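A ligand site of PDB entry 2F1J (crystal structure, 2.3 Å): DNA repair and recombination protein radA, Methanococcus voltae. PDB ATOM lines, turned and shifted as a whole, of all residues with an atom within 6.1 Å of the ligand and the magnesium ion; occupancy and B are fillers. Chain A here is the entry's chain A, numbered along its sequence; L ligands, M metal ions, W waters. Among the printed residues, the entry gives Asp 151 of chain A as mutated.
O4 of the ligand lies within hydrogen-bond range of N of Thr 112 (3.0 Å). N of Lys 111 sits at hydrogen-bond distance from O2 of the ligand (2.7 Å). The side-chain amino group (NZ) of Lys 111 lies within salt-bridge range of an oxygen (O2) of the ligand (2.6 Å). An oxygen (O3) of the ligand is in hydrogen-bond range of the backbone NH (N) of Gly 108, 2.7 Å away. An oxygen (O4) of the ligand sits at hydrogen-bond distance from the backbone NH (N) of Gln 113 (2.9 Å). NE2 of Gln 113 lies close to O4 of the ligand, 3.4 Å away. N of Gly 110 is in hydrogen-bond range of O2 of the ligand (2.9 Å). OE1 of Gln 161 is in hydrogen-bond range of N3 of the ligand (3.0 Å). N of Ser 109 sits at hydrogen-bond distance from O2 of the ligand (3.4 Å). OG of Ser 109 is in hydrogen-bond range of O2 of the ligand (3.4 Å).
Water W3 bridges OD2 of Asp 151 (2.7 Å) and OG1 of Thr 153 (3.0 Å). Water W2 lies within hydrogen-bond range of an oxygen (O10) of the ligand (2.6 Å), the backbone carbonyl oxygen (O) of Ile 315 (2.9 Å) and the side-chain carboxylate (OD1) of Asp 294 (3.5 Å).
NZ of Lys 111 sits close to NE2 of Gln 257, 3.0 Å away. The side-chain amino group (NZ) of Lys 111 is in hydrogen-bond range of the backbone carbonyl oxygen (O) of Gly 105 (3.4 Å). The side-chain amide oxygen of Gln 257 is in hydrogen-bond range of the backbone NH of Phe 107, 2.6 Å away. NH1 of Arg 158 sits at hydrogen-bond distance from O of Thr 316. The guanidinium group of Arg 158 sits at hydrogen-bond distance from the backbone carbonyl oxygen of Glu 317, 3.1 Å away. The guanidinium group (NH1) of Arg 296 lies within hydrogen-bond range of the backbone carbonyl oxygen (O) of Asp 294 (3.3 Å). NH1 of Arg 296 sits at hydrogen-bond distance from O of Gly 293, 2.9 Å away. The backbone carbonyl oxygen of Asp 294 is in hydrogen-bond range of the backbone NH of Ile 315.
N3 of the ligand lies close to NH2 of Arg 158, 3.3 Å away. O of Val 106 touches O2 of the ligand (3.8 Å). Phe 107 touches the ligand (CD2 to O3, 2.9 Å). Arg 296 touches the ligand (NH2 to O10, 3.7 Å). CG2 of Ile 315 touches C5 of the ligand, 3.8 Å away. Thr 316 touches the ligand (C to C9, 3.4 Å). CA of Glu 317 touches N4 of the ligand, at 3.5 Å.
The magnesium ion is bound by water W1 (1.9 Å), O1 of the ligand (2.0 Å), water W3 (2.1 Å), water W5 (2.1 Å), OG1 of Thr 112 (2.2 Å) and water W6 (2.2 Å).
Of the 24 residues printed, 1 comes within 4 Å of the magnesium ion. The nearest printed residue that does not touch the magnesium ion is Asp 211 (4.2 Å).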
ATOM      1  N   GLY A 105     -24.051   3.722 -35.446  1.00  0.00           N
ATOM      2  CA  GLY A 105     -23.637   2.352 -35.191  1.00  0.00           C
ATOM      3  C   GLY A 105     -24.780   1.497 -34.710  1.00  0.00           C
ATOM      4  O   GLY A 105     -25.888   1.998 -34.478  1.00  0.00           O
ATOM      5  N   VAL A 106     -24.523   0.195 -34.557  1.00  0.00           N
ATOM      6  CA  VAL A 106     -25.559  -0.722 -34.105  1.00  0.00           C
ATOM      7  C   VAL A 106     -25.934  -0.475 -32.655  1.00  0.00           C
ATOM      8  O   VAL A 106     -25.217   0.190 -31.900  1.00  0.00           O
ATOM      9  CB  VAL A 106     -25.116  -2.196 -34.259  1.00  0.00           C
ATOM     10  CG1 VAL A 106     -24.816  -2.485 -35.739  1.00  0.00           C
ATOM     11  CG2 VAL A 106     -23.904  -2.476 -33.388  1.00  0.00           C
ATOM     12  N   PHE A 107     -27.077  -1.030 -32.259  1.00  0.00           N
ATOM     13  CA  PHE A 107     -27.518  -0.871 -30.898  1.00  0.00           C
ATOM     14  C   PHE A 107     -26.466  -1.531 -30.008  1.00  0.00           C
ATOM     15  O   PHE A 107     -26.024  -2.652 -30.283  1.00  0.00           O
ATOM     16  CB  PHE A 107     -28.896  -1.522 -30.700  1.00  0.00           C
ATOM     17  CG  PHE A 107     -29.613  -1.057 -29.448  1.00  0.00           C
ATOM     18  CD1 PHE A 107     -31.000  -1.047 -29.401  1.00  0.00           C
ATOM     19  CD2 PHE A 107     -28.900  -0.672 -28.313  1.00  0.00           C
ATOM     20  CE1 PHE A 107     -31.684  -0.641 -28.239  1.00  0.00           C
ATOM     21  CE2 PHE A 107     -29.559  -0.266 -27.147  1.00  0.00           C
ATOM     22  CZ  PHE A 107     -30.950  -0.248 -27.104  1.00  0.00           C
ATOM     23  N   GLY A 108     -26.044  -0.828 -28.970  1.00  0.00           N
ATOM     24  CA  GLY A 108     -25.069  -1.369 -28.054  1.00  0.00           C
ATOM     25  C   GLY A 108     -23.636  -1.012 -28.372  1.00  0.00           C
ATOM     26  O   GLY A 108     -22.732  -1.361 -27.618  1.00  0.00           O
ATOM     27  N   SER A 109     -23.421  -0.310 -29.481  1.00  0.00           N
ATOM     28  CA  SER A 109     -22.059   0.058 -29.871  1.00  0.00           C
ATOM     29  C   SER A 109     -21.441   1.127 -28.971  1.00  0.00           C
ATOM     30  O   SER A 109     -20.233   1.275 -28.968  1.00  0.00           O
ATOM     31  CB  SER A 109     -22.037   0.523 -31.330  1.00  0.00           C
ATOM     32  OG  SER A 109     -22.872   1.644 -31.529  1.00  0.00           O
ATOM     33  N   GLY A 110     -22.262   1.867 -28.230  1.00  0.00           N
ATOM     34  CA  GLY A 110     -21.728   2.880 -27.327  1.00  0.00           C
ATOM     35  C   GLY A 110     -22.091   4.340 -27.611  1.00  0.00           C
ATOM     36  O   GLY A 110     -21.512   5.255 -27.011  1.00  0.00           O
ATOM     37  N   LYS A 111     -23.057   4.558 -28.504  1.00  0.00           N
ATOM     38  CA  LYS A 111     -23.463   5.922 -28.861  1.00  0.00           C
ATOM     39  C   LYS A 111     -23.884   6.718 -27.629  1.00  0.00           C
ATOM     40  O   LYS A 111     -23.332   7.787 -27.349  1.00  0.00           O
ATOM     41  CB  LYS A 111     -24.606   5.875 -29.887  1.00  0.00           C
ATOM     42  CG  LYS A 111     -24.258   5.080 -31.131  1.00  0.00           C
ATOM     43  CD  LYS A 111     -25.376   5.115 -32.177  1.00  0.00           C
ATOM     44  CE  LYS A 111     -26.616   4.395 -31.697  1.00  0.00           C
ATOM     45  NZ  LYS A 111     -26.270   3.024 -31.270  1.00  0.00           N
ATOM     46  N   THR A 112     -24.853   6.207 -26.886  1.00  0.00           N
ATOM     47  CA  THR A 112     -25.340   6.891 -25.690  1.00  0.00           C
ATOM     48  C   THR A 112     -24.227   7.073 -24.646  1.00  0.00           C
ATOM     49  O   THR A 112     -24.164   8.109 -23.957  1.00  0.00           O
ATOM     50  CB  THR A 112     -26.541   6.095 -25.099  1.00  0.00           C
ATOM     51  OG1 THR A 112     -27.624   6.137 -26.052  1.00  0.00           O
ATOM     52  CG2 THR A 112     -27.011   6.687 -23.781  1.00  0.00           C
ATOM     53  N   GLN A 113     -23.338   6.094 -24.544  1.00  0.00           N
ATOM     54  CA  GLN A 113     -22.209   6.164 -23.616  1.00  0.00           C
ATOM     55  C   GLN A 113     -21.365   7.402 -23.921  1.00  0.00           C
ATOM     56  O   GLN A 113     -21.041   8.170 -23.018  1.00  0.00           O
ATOM     57  CB  GLN A 113     -21.344   4.912 -23.726  1.00  0.00           C
ATOM     58  CG  GLN A 113     -22.074   3.629 -23.387  1.00  0.00           C
ATOM     59  CD  GLN A 113     -22.769   3.713 -22.047  1.00  0.00           C
ATOM     60  OE1 GLN A 113     -22.115   3.861 -21.007  1.00  0.00           O
ATOM     61  NE2 GLN A 113     -24.108   3.650 -22.052  1.00  0.00           N
ATOM     62  N   ILE A 114     -21.005   7.576 -25.185  1.00  0.00           N
ATOM     63  CA  ILE A 114     -20.181   8.720 -25.584  1.00  0.00           C
ATOM     64  C   ILE A 114     -20.919  10.013 -25.254  1.00  0.00           C
ATOM     65  O   ILE A 114     -20.289  10.985 -24.812  1.00  0.00           O
ATOM     66  CB  ILE A 114     -19.832   8.647 -27.092  1.00  0.00           C
ATOM     67  CG1 ILE A 114     -18.895   7.466 -27.347  1.00  0.00           C
ATOM     68  CG2 ILE A 114     -19.192   9.925 -27.548  1.00  0.00           C
ATOM     69  CD1 ILE A 114     -18.665   7.162 -28.822  1.00  0.00           C
ATOM     70  N   ASP A 151     -34.590   8.817 -26.897  1.00  0.00           N
ATOM     71  CA  ASP A 151     -34.878   7.407 -26.647  1.00  0.00           C
ATOM     72  C   ASP A 151     -35.284   7.130 -25.203  1.00  0.00           C
ATOM     73  O   ASP A 151     -35.761   6.036 -24.876  1.00  0.00           O
ATOM     74  CB  ASP A 151     -33.659   6.535 -26.986  1.00  0.00           C
ATOM     75  CG  ASP A 151     -33.131   6.795 -28.396  1.00  0.00           C
ATOM     76  OD1 ASP A 151     -33.936   7.082 -29.305  1.00  0.00           O
ATOM     77  OD2 ASP A 151     -31.896   6.697 -28.588  1.00  0.00           O
ATOM     78  N   THR A 153     -33.110   7.211 -22.669  1.00  0.00           N
ATOM     79  CA  THR A 153     -32.039   6.444 -22.050  1.00  0.00           C
ATOM     80  C   THR A 153     -31.023   7.267 -21.260  1.00  0.00           C
ATOM     81  O   THR A 153     -29.930   6.787 -20.964  1.00  0.00           O
ATOM     82  CB  THR A 153     -31.290   5.575 -23.082  1.00  0.00           C
ATOM     83  OG1 THR A 153     -30.955   6.359 -24.221  1.00  0.00           O
ATOM     84  CG2 THR A 153     -32.177   4.379 -23.510  1.00  0.00           C
ATOM     85  N   ARG A 158     -25.262   6.829 -14.414  1.00  0.00           N
ATOM     86  CA  ARG A 158     -24.093   6.712 -15.272  1.00  0.00           C
ATOM     87  C   ARG A 158     -23.280   7.999 -15.269  1.00  0.00           C
ATOM     88  O   ARG A 158     -22.057   7.968 -15.347  1.00  0.00           O
ATOM     89  CB  ARG A 158     -24.518   6.322 -16.689  1.00  0.00           C
ATOM     90  CG  ARG A 158     -23.378   5.964 -17.623  1.00  0.00           C
ATOM     91  CD  ARG A 158     -22.512   4.797 -17.095  1.00  0.00           C
ATOM     92  NE  ARG A 158     -21.679   4.260 -18.163  1.00  0.00           N
ATOM     93  CZ  ARG A 158     -20.519   3.623 -18.001  1.00  0.00           C
ATOM     94  NH1 ARG A 158     -19.863   3.177 -19.067  1.00  0.00           N
ATOM     95  NH2 ARG A 158     -19.994   3.456 -16.789  1.00  0.00           N
ATOM     96  N   GLN A 161     -21.379   7.960 -12.001  1.00  0.00           N
ATOM     97  CA  GLN A 161     -20.319   6.977 -12.041  1.00  0.00           C
ATOM     98  C   GLN A 161     -19.116   7.471 -12.881  1.00  0.00           C
ATOM     99  O   GLN A 161     -17.984   7.491 -12.401  1.00  0.00           O
ATOM    100  CB  GLN A 161     -20.850   5.652 -12.589  1.00  0.00           C
ATOM    101  CG  GLN A 161     -19.820   4.566 -12.764  1.00  0.00           C
ATOM    102  CD  GLN A 161     -20.407   3.273 -13.318  1.00  0.00           C
ATOM    103  OE1 GLN A 161     -21.095   3.269 -14.343  1.00  0.00           O
ATOM    104  NE2 GLN A 161     -20.122   2.171 -12.638  1.00  0.00           N
ATOM    105  N   ASP A 211     -29.715  12.610 -28.686  1.00  0.00           N
ATOM    106  CA  ASP A 211     -29.661  11.154 -28.675  1.00  0.00           C
ATOM    107  C   ASP A 211     -31.060  10.521 -28.578  1.00  0.00           C
ATOM    108  O   ASP A 211     -31.637  10.459 -27.498  1.00  0.00           O
ATOM    109  CB  ASP A 211     -28.770  10.711 -27.504  1.00  0.00           C
ATOM    110  CG  ASP A 211     -28.614   9.206 -27.407  1.00  0.00           C
ATOM    111  OD1 ASP A 211     -28.516   8.541 -28.463  1.00  0.00           O
ATOM    112  OD2 ASP A 211     -28.570   8.688 -26.270  1.00  0.00           O
ATOM    113  N   THR A 255     -26.530  11.209 -32.416  1.00  0.00           N
ATOM    114  CA  THR A 255     -26.327   9.782 -32.615  1.00  0.00           C
ATOM    115  C   THR A 255     -27.327   9.282 -33.641  1.00  0.00           C
ATOM    116  O   THR A 255     -28.414   9.843 -33.803  1.00  0.00           O
ATOM    117  CB  THR A 255     -26.493   9.004 -31.293  1.00  0.00           C
ATOM    118  OG1 THR A 255     -27.869   9.020 -30.915  1.00  0.00           O
ATOM    119  CG2 THR A 255     -25.629   9.661 -30.177  1.00  0.00           C
ATOM    120  N   GLN A 257     -28.863   5.490 -35.124  1.00  0.00           N
ATOM    121  CA  GLN A 257     -28.925   4.046 -35.058  1.00  0.00           C
ATOM    122  C   GLN A 257     -28.857   3.495 -36.500  1.00  0.00           C
ATOM    123  O   GLN A 257     -29.575   3.961 -37.370  1.00  0.00           O
ATOM    124  CB  GLN A 257     -30.231   3.606 -34.402  1.00  0.00           C
ATOM    125  CG  GLN A 257     -30.356   2.104 -34.224  1.00  0.00           C
ATOM    126  CD  GLN A 257     -29.331   1.546 -33.260  1.00  0.00           C
ATOM    127  OE1 GLN A 257     -28.770   0.475 -33.501  1.00  0.00           O
ATOM    128  NE2 GLN A 257     -29.082   2.271 -32.169  1.00  0.00           N
ATOM    129  N   GLY A 293     -15.728  -7.982 -26.411  1.00  0.00           N
ATOM    130  CA  GLY A 293     -16.056  -7.561 -25.057  1.00  0.00           C
ATOM    131  C   GLY A 293     -16.121  -6.059 -24.840  1.00  0.00           C
ATOM    132  O   GLY A 293     -17.020  -5.387 -25.356  1.00  0.00           O
ATOM    133  N   ASP A 294     -15.165  -5.542 -24.087  1.00  0.00           N
ATOM    134  CA  ASP A 294     -15.078  -4.106 -23.785  1.00  0.00           C
ATOM    135  C   ASP A 294     -14.787  -3.281 -25.033  1.00  0.00           C
ATOM    136  O   ASP A 294     -15.294  -2.161 -25.162  1.00  0.00           O
ATOM    137  CB  ASP A 294     -13.963  -3.834 -22.779  1.00  0.00           C
ATOM    138  CG  ASP A 294     -14.451  -3.795 -21.357  1.00  0.00           C
ATOM    139  OD1 ASP A 294     -15.523  -3.217 -21.114  1.00  0.00           O
ATOM    140  OD2 ASP A 294     -13.756  -4.336 -20.478  1.00  0.00           O
ATOM    141  N   ARG A 296     -14.318  -1.435 -28.621  1.00  0.00           N
ATOM    142  CA  ARG A 296     -15.186  -0.727 -29.544  1.00  0.00           C
ATOM    143  C   ARG A 296     -14.294  -0.105 -30.608  1.00  0.00           C
ATOM    144  O   ARG A 296     -13.176   0.313 -30.323  1.00  0.00           O
ATOM    145  CB  ARG A 296     -15.939   0.385 -28.808  1.00  0.00           C
ATOM    146  CG  ARG A 296     -16.889  -0.095 -27.709  1.00  0.00           C
ATOM    147  CD  ARG A 296     -18.120  -0.754 -28.294  1.00  0.00           C
ATOM    148  NE  ARG A 296     -19.079  -1.103 -27.258  1.00  0.00           N
ATOM    149  CZ  ARG A 296     -19.019  -2.196 -26.509  1.00  0.00           C
ATOM    150  NH1 ARG A 296     -18.047  -3.079 -26.694  1.00  0.00           N
ATOM    151  NH2 ARG A 296     -19.931  -2.406 -25.574  1.00  0.00           N
ATOM    152  N   ILE A 315     -15.286   0.537 -23.289  1.00  0.00           N
ATOM    153  CA  ILE A 315     -16.314   1.070 -22.432  1.00  0.00           C
ATOM    154  C   ILE A 315     -16.374   0.246 -21.155  1.00  0.00           C
ATOM    155  O   ILE A 315     -16.784  -0.915 -21.158  1.00  0.00           O
ATOM    156  CB  ILE A 315     -17.698   1.034 -23.122  1.00  0.00           C
ATOM    157  CG1 ILE A 315     -17.681   1.893 -24.385  1.00  0.00           C
ATOM    158  CG2 ILE A 315     -18.782   1.513 -22.148  1.00  0.00           C
ATOM    159  CD1 ILE A 315     -18.996   1.875 -25.178  1.00  0.00           C
ATOM    160  N   THR A 316     -15.934   0.844 -20.052  1.00  0.00           N
ATOM    161  CA  THR A 316     -15.918   0.167 -18.773  1.00  0.00           C
ATOM    162  C   THR A 316     -16.759   0.955 -17.789  1.00  0.00           C
ATOM    163  O   THR A 316     -17.503   1.864 -18.194  1.00  0.00           O
ATOM    164  CB  THR A 316     -14.504   0.096 -18.227  1.00  0.00           C
ATOM    165  OG1 THR A 316     -14.053   1.419 -17.935  1.00  0.00           O
ATOM    166  CG2 THR A 316     -13.574  -0.540 -19.263  1.00  0.00           C
ATOM    167  N   GLU A 317     -16.639   0.631 -16.513  1.00  0.00           N
ATOM    168  CA  GLU A 317     -17.398   1.333 -15.484  1.00  0.00           C
ATOM    169  C   GLU A 317     -16.937   2.777 -15.350  1.00  0.00           C
ATOM    170  O   GLU A 317     -17.632   3.603 -14.770  1.00  0.00           O
ATOM    171  CB  GLU A 317     -17.270   0.617 -14.127  1.00  0.00           C
ATOM    172  CG  GLU A 317     -16.212  -0.495 -14.061  1.00  0.00           C
ATOM    173  CD  GLU A 317     -14.797   0.037 -13.951  1.00  0.00           C
ATOM    174  OE1 GLU A 317     -14.486   0.716 -12.945  1.00  0.00           O
ATOM    175  OE2 GLU A 317     -13.992  -0.232 -14.876  1.00  0.00           O
ATOM    176  N   LYS A 318     -15.763   3.076 -15.888  1.00  0.00           N
ATOM    177  CA  LYS A 318     -15.224   4.432 -15.821  1.00  0.00           C
ATOM    178  C   LYS A 318     -15.740   5.298 -16.974  1.00  0.00           C
ATOM    179  O   LYS A 318     -15.559   6.517 -16.973  1.00  0.00           O
ATOM    180  CB  LYS A 318     -13.695   4.393 -15.879  1.00  0.00           C
ATOM    181  CG  LYS A 318     -13.047   3.620 -14.739  1.00  0.00           C
ATOM    182  CD  LYS A 318     -11.531   3.604 -14.895  1.00  0.00           C
ATOM    183  CE  LYS A 318     -10.863   3.042 -13.657  1.00  0.00           C
ATOM    184  NZ  LYS A 318     -11.310   1.644 -13.367  1.00  0.00           N
HETATM  185  P1  LIG L   1     -25.984   2.444 -28.001  1.00  0.00           P
HETATM  186  O1  LIG L   1     -26.477   3.751 -27.514  1.00  0.00           O
HETATM  187  O2  LIG L   1     -24.963   2.661 -29.023  1.00  0.00           O
HETATM  188  O3  LIG L   1     -27.209   1.613 -28.613  1.00  0.00           O
HETATM  189  P2  LIG L   1     -25.048   2.175 -25.348  1.00  0.00           P
HETATM  190  O4  LIG L   1     -24.458   3.588 -25.438  1.00  0.00           O
HETATM  191  O5  LIG L   1     -26.309   2.198 -24.571  1.00  0.00           O
HETATM  192  O6  LIG L   1     -25.328   1.578 -26.817  1.00  0.00           O
HETATM  193  O7  LIG L   1     -23.941   1.199 -24.599  1.00  0.00           O
HETATM  194  C1  LIG L   1     -24.246  -0.220 -24.190  1.00  0.00           C
HETATM  195  C2  LIG L   1     -23.133  -0.752 -23.655  1.00  0.00           C
HETATM  196  O8  LIG L   1     -22.590   0.189 -22.662  1.00  0.00           O
HETATM  197  C3  LIG L   1     -23.504  -1.975 -22.779  1.00  0.00           C
HETATM  198  O9  LIG L   1     -23.967  -3.071 -23.478  1.00  0.00           O
HETATM  199  C4  LIG L   1     -22.395  -2.022 -21.701  1.00  0.00           C
HETATM  200  O10 LIG L   1     -21.285  -2.958 -22.221  1.00  0.00           O
HETATM  201  C5  LIG L   1     -21.879  -0.584 -21.662  1.00  0.00           C
HETATM  202  N1  LIG L   1     -22.124  -0.095 -20.445  1.00  0.00           N
HETATM  203  C6  LIG L   1     -23.240   0.676 -20.033  1.00  0.00           C
HETATM  204  N2  LIG L   1     -23.130   0.941 -18.777  1.00  0.00           N
HETATM  205  C7  LIG L   1     -21.993   0.396 -18.296  1.00  0.00           C
HETATM  206  C8  LIG L   1     -21.396   0.362 -17.059  1.00  0.00           C
HETATM  207  N3  LIG L   1     -21.986   0.980 -16.003  1.00  0.00           N
HETATM  208  N4  LIG L   1     -20.161  -0.328 -16.900  1.00  0.00           N
HETATM  209  C9  LIG L   1     -19.539  -0.976 -18.003  1.00  0.00           C
HETATM  210  N5  LIG L   1     -20.107  -0.966 -19.241  1.00  0.00           N
HETATM  211  C10 LIG L   1     -21.343  -0.264 -19.342  1.00  0.00           C
HETATM  212 MG    MG M   1     -28.305   4.546 -27.329  1.00  0.00          MG
HETATM  213  O   HOH W   1     -29.190   3.149 -28.313  1.00  0.00           O
HETATM  214  O   HOH W   2     -18.958  -2.789 -21.071  1.00  0.00           O
HETATM  215  O   HOH W   3     -30.285   5.224 -26.923  1.00  0.00           O
HETATM  216  O   HOH W   4     -28.484   0.217 -24.190  1.00  0.00           O
HETATM  217  O   HOH W   5     -28.222   3.528 -25.445  1.00  0.00           O
HETATM  218  O   HOH W   6     -28.271   5.884 -29.033  1.00  0.00           O
